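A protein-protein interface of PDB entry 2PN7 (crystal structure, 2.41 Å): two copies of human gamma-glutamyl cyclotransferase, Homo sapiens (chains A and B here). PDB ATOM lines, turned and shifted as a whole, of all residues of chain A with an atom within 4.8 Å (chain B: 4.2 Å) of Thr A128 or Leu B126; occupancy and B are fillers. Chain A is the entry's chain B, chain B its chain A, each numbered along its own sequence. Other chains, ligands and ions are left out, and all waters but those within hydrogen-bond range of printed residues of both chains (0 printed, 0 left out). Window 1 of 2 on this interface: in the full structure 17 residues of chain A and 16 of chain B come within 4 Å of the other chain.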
ATOM      1  N   GLN A  73      10.969  13.462 -29.591  1.00  0.00           N
ATOM      2  CA  GLN A  73      10.194  12.252 -29.366  1.00  0.00           C
ATOM      3  C   GLN A  73      10.162  11.469 -30.654  1.00  0.00           C
ATOM      4  O   GLN A  73       9.854  12.007 -31.720  1.00  0.00           O
ATOM      5  CB  GLN A  73       8.784  12.585 -28.845  1.00  0.00           C
ATOM      6  CG  GLN A  73       8.810  13.097 -27.375  1.00  0.00           C
ATOM      7  CD  GLN A  73       7.531  13.807 -26.956  1.00  0.00           C
ATOM      8  OE1 GLN A  73       7.057  14.742 -27.636  1.00  0.00           O
ATOM      9  NE2 GLN A  73       6.952  13.366 -25.836  1.00  0.00           N
ATOM     10  N   VAL A 106      14.858  24.755 -24.374  1.00  0.00           N
ATOM     11  CA  VAL A 106      13.785  24.837 -23.390  1.00  0.00           C
ATOM     12  C   VAL A 106      14.091  23.811 -22.284  1.00  0.00           C
ATOM     13  O   VAL A 106      14.712  22.785 -22.572  1.00  0.00           O
ATOM     14  CB  VAL A 106      12.366  24.593 -24.070  1.00  0.00           C
ATOM     15  CG1 VAL A 106      12.147  23.110 -24.376  1.00  0.00           C
ATOM     16  CG2 VAL A 106      11.232  25.116 -23.206  1.00  0.00           C
ATOM     17  N   LEU A 126      16.035  20.684 -24.381  1.00  0.00           N
ATOM     18  CA  LEU A 126      16.020  20.372 -25.801  1.00  0.00           C
ATOM     19  C   LEU A 126      15.771  21.654 -26.607  1.00  0.00           C
ATOM     20  O   LEU A 126      15.197  22.603 -26.075  1.00  0.00           O
ATOM     21  CB  LEU A 126      15.019  19.230 -26.154  1.00  0.00           C
ATOM     22  CG  LEU A 126      13.513  19.283 -25.794  1.00  0.00           C
ATOM     23  CD1 LEU A 126      12.690  20.258 -26.622  1.00  0.00           C
ATOM     24  CD2 LEU A 126      12.893  17.900 -25.891  1.00  0.00           C
ATOM     25  N   MET A 127      16.269  21.680 -27.853  1.00  0.00           N
ATOM     26  CA  MET A 127      15.948  22.737 -28.831  1.00  0.00           C
ATOM     27  C   MET A 127      14.536  22.558 -29.426  1.00  0.00           C
ATOM     28  O   MET A 127      14.117  21.433 -29.699  1.00  0.00           O
ATOM     29  CB  MET A 127      16.967  22.778 -29.967  1.00  0.00           C
ATOM     30  CG  MET A 127      18.442  22.757 -29.535  1.00  0.00           C
ATOM     31  SD  MET A 127      19.538  23.636 -30.694  1.00  0.00           S
ATOM     32  CE  MET A 127      19.913  22.286 -31.788  1.00  0.00           C
ATOM     33  N   THR A 128      13.815  23.665 -29.603  1.00  0.00           N
ATOM     34  CA  THR A 128      12.506  23.664 -30.243  1.00  0.00           C
ATOM     35  C   THR A 128      12.546  24.270 -31.660  1.00  0.00           C
ATOM     36  O   THR A 128      11.635  24.084 -32.469  1.00  0.00           O
ATOM     37  CB  THR A 128      11.492  24.486 -29.435  1.00  0.00           C
ATOM     38  OG1 THR A 128      11.857  25.874 -29.487  1.00  0.00           O
ATOM     39  CG2 THR A 128      11.428  23.999 -27.981  1.00  0.00           C
ATOM     40  N   ASN A 129      13.584  25.034 -31.943  1.00  0.00           N
ATOM     41  CA  ASN A 129      13.680  25.716 -33.226  1.00  0.00           C
ATOM     42  C   ASN A 129      15.131  25.663 -33.646  1.00  0.00           C
ATOM     43  O   ASN A 129      15.945  26.482 -33.228  1.00  0.00           O
ATOM     44  CB  ASN A 129      13.160  27.154 -33.122  1.00  0.00           C
ATOM     45  CG  ASN A 129      12.781  27.748 -34.470  1.00  0.00           C
ATOM     46  OD1 ASN A 129      12.967  27.127 -35.516  1.00  0.00           O
ATOM     47  ND2 ASN A 129      12.229  28.968 -34.447  1.00  0.00           N
ATOM     48  N   TYR A 130      15.450  24.652 -34.438  1.00  0.00           N
ATOM     49  CA  TYR A 130      16.785  24.504 -34.957  1.00  0.00           C
ATOM     50  C   TYR A 130      16.716  23.961 -36.374  1.00  0.00           C
ATOM     51  O   TYR A 130      15.688  23.442 -36.808  1.00  0.00           O
ATOM     52  CB  TYR A 130      17.604  23.576 -34.059  1.00  0.00           C
ATOM     53  CG  TYR A 130      17.160  22.127 -34.077  1.00  0.00           C
ATOM     54  CD1 TYR A 130      16.043  21.690 -33.336  1.00  0.00           C
ATOM     55  CD2 TYR A 130      17.849  21.186 -34.836  1.00  0.00           C
ATOM     56  CE1 TYR A 130      15.633  20.358 -33.379  1.00  0.00           C
ATOM     57  CE2 TYR A 130      17.449  19.857 -34.877  1.00  0.00           C
ATOM     58  CZ  TYR A 130      16.353  19.450 -34.160  1.00  0.00           C
ATOM     59  OH  TYR A 130      15.996  18.123 -34.213  1.00  0.00           O
ATOM     60  N   TYR B  22      -2.273  27.067 -23.067  1.00  0.00           N
ATOM     61  CA  TYR B  22      -2.297  28.018 -24.186  1.00  0.00           C
ATOM     62  C   TYR B  22      -3.191  27.552 -25.330  1.00  0.00           C
ATOM     63  O   TYR B  22      -3.408  28.288 -26.293  1.00  0.00           O
ATOM     64  CB  TYR B  22      -0.884  28.316 -24.695  1.00  0.00           C
ATOM     65  CG  TYR B  22      -0.123  27.073 -25.043  1.00  0.00           C
ATOM     66  CD1 TYR B  22      -0.350  26.422 -26.263  1.00  0.00           C
ATOM     67  CD2 TYR B  22       0.813  26.522 -24.146  1.00  0.00           C
ATOM     68  CE1 TYR B  22       0.325  25.237 -26.590  1.00  0.00           C
ATOM     69  CE2 TYR B  22       1.526  25.348 -24.483  1.00  0.00           C
ATOM     70  CZ  TYR B  22       1.263  24.723 -25.714  1.00  0.00           C
ATOM     71  OH  TYR B  22       1.891  23.569 -26.063  1.00  0.00           O
ATOM     72  N   THR B  70       0.465  23.945 -30.031  1.00  0.00           N
ATOM     73  CA  THR B  70       1.863  23.776 -29.609  1.00  0.00           C
ATOM     74  C   THR B  70       2.625  25.125 -29.670  1.00  0.00           C
ATOM     75  O   THR B  70       2.154  26.099 -30.231  1.00  0.00           O
ATOM     76  CB  THR B  70       2.589  22.686 -30.453  1.00  0.00           C
ATOM     77  OG1 THR B  70       3.918  22.438 -29.941  1.00  0.00           O
ATOM     78  CG2 THR B  70       2.647  23.076 -31.952  1.00  0.00           C
ATOM     79  N   ILE B  71       3.807  25.171 -29.079  1.00  0.00           N
ATOM     80  CA  ILE B  71       4.589  26.390 -29.049  1.00  0.00           C
ATOM     81  C   ILE B  71       5.995  26.045 -29.346  1.00  0.00           C
ATOM     82  O   ILE B  71       6.437  24.933 -29.043  1.00  0.00           O
ATOM     83  CB  ILE B  71       4.534  27.152 -27.655  1.00  0.00           C
ATOM     84  CG1 ILE B  71       4.808  26.207 -26.482  1.00  0.00           C
ATOM     85  CG2 ILE B  71       3.224  27.948 -27.489  1.00  0.00           C
ATOM     86  CD1 ILE B  71       4.785  26.894 -25.097  1.00  0.00           C
ATOM     87  N   PHE B  72       6.712  27.000 -29.918  1.00  0.00           N
ATOM     88  CA  PHE B  72       8.159  26.866 -30.072  1.00  0.00           C
ATOM     89  C   PHE B  72       8.879  28.228 -29.909  1.00  0.00           C
ATOM     90  O   PHE B  72       8.266  29.304 -30.046  1.00  0.00           O
ATOM     91  CB  PHE B  72       8.500  26.170 -31.397  1.00  0.00           C
ATOM     92  CG  PHE B  72       8.039  26.922 -32.622  1.00  0.00           C
ATOM     93  CD1 PHE B  72       8.875  27.866 -33.233  1.00  0.00           C
ATOM     94  CD2 PHE B  72       6.779  26.695 -33.159  1.00  0.00           C
ATOM     95  CE1 PHE B  72       8.466  28.577 -34.357  1.00  0.00           C
ATOM     96  CE2 PHE B  72       6.351  27.408 -34.298  1.00  0.00           C
ATOM     97  CZ  PHE B  72       7.202  28.340 -34.897  1.00  0.00           C
ATOM     98  N   GLN B  73      10.173  28.181 -29.601  1.00  0.00           N
ATOM     99  CA  GLN B  73      10.904  29.405 -29.324  1.00  0.00           C
ATOM    100  C   GLN B  73      11.090  30.219 -30.586  1.00  0.00           C
ATOM    101  O   GLN B  73      11.374  29.680 -31.645  1.00  0.00           O
ATOM    102  CB  GLN B  73      12.222  29.127 -28.621  1.00  0.00           C
ATOM    103  CG  GLN B  73      12.022  28.793 -27.145  1.00  0.00           C
ATOM    104  CD  GLN B  73      13.083  27.846 -26.613  1.00  0.00           C
ATOM    105  OE1 GLN B  73      13.264  26.755 -27.158  1.00  0.00           O
ATOM    106  NE2 GLN B  73      13.787  28.255 -25.539  1.00  0.00           N
ATOM    107  N   TYR B 105       3.338  15.046 -26.546  1.00  0.00           N
ATOM    108  CA  TYR B 105       3.902  16.244 -25.959  1.00  0.00           C
ATOM    109  C   TYR B 105       5.022  15.884 -25.003  1.00  0.00           C
ATOM    110  O   TYR B 105       5.107  14.754 -24.508  1.00  0.00           O
ATOM    111  CB  TYR B 105       2.848  17.027 -25.196  1.00  0.00           C
ATOM    112  CG  TYR B 105       1.807  17.732 -26.034  1.00  0.00           C
ATOM    113  CD1 TYR B 105       0.634  17.080 -26.423  1.00  0.00           C
ATOM    114  CD2 TYR B 105       1.963  19.063 -26.399  1.00  0.00           C
ATOM    115  CE1 TYR B 105      -0.351  17.733 -27.197  1.00  0.00           C
ATOM    116  CE2 TYR B 105       0.972  19.741 -27.156  1.00  0.00           C
ATOM    117  CZ  TYR B 105      -0.174  19.068 -27.541  1.00  0.00           C
ATOM    118  OH  TYR B 105      -1.148  19.722 -28.269  1.00  0.00           O
ATOM    119  N   VAL B 106       5.919  16.842 -24.786  1.00  0.00           N
ATOM    120  CA  VAL B 106       6.965  16.691 -23.792  1.00  0.00           C
ATOM    121  C   VAL B 106       6.636  17.655 -22.648  1.00  0.00           C
ATOM    122  O   VAL B 106       6.088  18.725 -22.884  1.00  0.00           O
ATOM    123  CB  VAL B 106       8.374  16.917 -24.414  1.00  0.00           C
ATOM    124  CG1 VAL B 106       8.596  18.369 -24.721  1.00  0.00           C
ATOM    125  CG2 VAL B 106       9.477  16.379 -23.501  1.00  0.00           C
ATOM    126  N   ILE B 108       7.432  20.559 -20.250  1.00  0.00           N
ATOM    127  CA  ILE B 108       8.343  21.693 -20.102  1.00  0.00           C
ATOM    128  C   ILE B 108       8.190  22.510 -18.770  1.00  0.00           C
ATOM    129  O   ILE B 108       7.182  22.400 -18.057  1.00  0.00           O
ATOM    130  CB  ILE B 108       8.270  22.647 -21.337  1.00  0.00           C
ATOM    131  CG1 ILE B 108       6.894  23.341 -21.459  1.00  0.00           C
ATOM    132  CG2 ILE B 108       8.668  21.912 -22.592  1.00  0.00           C
ATOM    133  CD1 ILE B 108       6.806  24.326 -22.640  1.00  0.00           C
ATOM    134  N   TYR B 125       3.458  22.129 -21.836  1.00  0.00           N
ATOM    135  CA  TYR B 125       3.735  21.070 -22.786  1.00  0.00           C
ATOM    136  C   TYR B 125       3.958  21.670 -24.153  1.00  0.00           C
ATOM    137  O   TYR B 125       3.411  22.737 -24.494  1.00  0.00           O
ATOM    138  CB  TYR B 125       2.553  20.118 -22.867  1.00  0.00           C
ATOM    139  CG  TYR B 125       2.242  19.484 -21.544  1.00  0.00           C
ATOM    140  CD1 TYR B 125       2.754  18.241 -21.224  1.00  0.00           C
ATOM    141  CD2 TYR B 125       1.428  20.127 -20.610  1.00  0.00           C
ATOM    142  CE1 TYR B 125       2.498  17.657 -20.002  1.00  0.00           C
ATOM    143  CE2 TYR B 125       1.144  19.527 -19.369  1.00  0.00           C
ATOM    144  CZ  TYR B 125       1.691  18.299 -19.084  1.00  0.00           C
ATOM    145  OH  TYR B 125       1.457  17.700 -17.879  1.00  0.00           O
ATOM    146  N   LEU B 126       4.792  20.995 -24.933  1.00  0.00           N
ATOM    147  CA  LEU B 126       4.856  21.287 -26.356  1.00  0.00           C
ATOM    148  C   LEU B 126       5.197  20.009 -27.106  1.00  0.00           C
ATOM    149  O   LEU B 126       5.595  19.026 -26.502  1.00  0.00           O
ATOM    150  CB  LEU B 126       5.835  22.437 -26.648  1.00  0.00           C
ATOM    151  CG  LEU B 126       7.324  22.315 -26.248  1.00  0.00           C
ATOM    152  CD1 LEU B 126       8.126  21.411 -27.163  1.00  0.00           C
ATOM    153  CD2 LEU B 126       7.969  23.692 -26.178  1.00  0.00           C
ATOM    154  N   MET B 127       5.006  20.036 -28.422  1.00  0.00           N
ATOM    155  CA  MET B 127       5.305  18.916 -29.292  1.00  0.00           C
ATOM    156  C   MET B 127       6.744  19.019 -29.816  1.00  0.00           C
ATOM    157  O   MET B 127       7.223  20.105 -30.164  1.00  0.00           O
ATOM    158  CB  MET B 127       4.333  18.887 -30.463  1.00  0.00           C
ATOM    159  CG  MET B 127       2.856  18.882 -30.110  1.00  0.00           C
ATOM    160  SD  MET B 127       1.935  18.307 -31.538  1.00  0.00           S
ATOM    161  CE  MET B 127       1.257  19.791 -32.175  1.00  0.00           C
ATOM    162  N   THR B 128       7.436  17.892 -29.861  1.00  0.00           N
ATOM    163  CA  THR B 128       8.822  17.890 -30.338  1.00  0.00           C
ATOM    164  C   THR B 128       8.947  17.287 -31.752  1.00  0.00           C
ATOM    165  O   THR B 128      10.013  17.346 -32.376  1.00  0.00           O
ATOM    166  CB  THR B 128       9.750  17.130 -29.348  1.00  0.00           C
ATOM    167  OG1 THR B 128       9.293  15.774 -29.188  1.00  0.00           O
ATOM    168  CG2 THR B 128       9.739  17.792 -28.012  1.00  0.00           C
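The backbone carbonyl oxygen (O) of Tyr B105 is in hydrogen-bond range of the side-chain amide nitrogen (NE2) of Gln A73 (2.7 Å).
The side-chain amide nitrogen (ND2) of Asn A129 lies within hydrogen-bond range of the backbone carbonyl oxygen (O) of Gln B73.
N of Gln B73 is in hydrogen-bond range of OG1 of Thr A128, 2.9 Å away.
OG1 of Thr B128 lies within hydrogen-bond range of N of Gln A73, at 2.9 Å.
The backbone NH (N) of Val B106 lies within hydrogen-bond range of the backbone carbonyl oxygen (O) of Leu B126, 2.8 Å away.
The backbone NH of Val A106 sits at hydrogen-bond distance from the backbone carbonyl oxygen of Leu A126 (2.8 Å).
Among the printed residues, pairs that only touch across the chains: Gln A73 with Val B106 (3.7 Å), Asn A129 with Phe B72 (3.7 Å), Val A106 with Gln B73 (3.8 Å), Leu A126 with Thr B128 (3.8 Å), Thr A128 with Phe B72 (3.8 Å) and Thr A128 with Leu B126 (3.9 Å).
Of the printed residues of chain B, Val A106 touches Gln B73 (3.8 Å).
Thr A128 touches three residues of chain B.
Of the printed residues of chain B, Asn A129 touches Phe B72 and Gln B73.
Ile B71 touches none of the printed residues of chain A.
Of chain A, only Thr A128 (3.9 Å) comes within 4 Å of Leu B126.
Met B127 touches none of the printed residues of chain A.
Printed residues of chain A within 4 Å of Thr B128: Gln A73 (2.9 Å) and Leu A126 (3.8 Å).
The nearest residue of chain A that does not touch Leu B126 is Val A106 (4.6 Å).
The nearest printed residue of chain A that does not touch Phe B72 is Met A127 (7.3 Å).
Printed residues of chain A that touch a printed residue of chain B: Gln A73, Val A106, Leu A126, Thr A128 and Asn A129.
Hydrophobic or aromatic side chains of chain A within 4 Å of the printed part of chain B: Val A106 and Leu A126.
Among the printed residues, 10 pairs touch across the chains.
Among the printed residues, no Asp or Glu carboxylate lies within 4 Å of a Lys or Arg side-chain nitrogen of the other chain.
Gln A73 touches Val B106, and with the chains exchanged Val A106 touches Gln B73.
Gln A73 touches Thr B128, and with the chains exchanged Thr A128 touches Gln B73.
Leu A126 touches Thr B128, and with the chains exchanged Thr A128 touches Leu B126.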
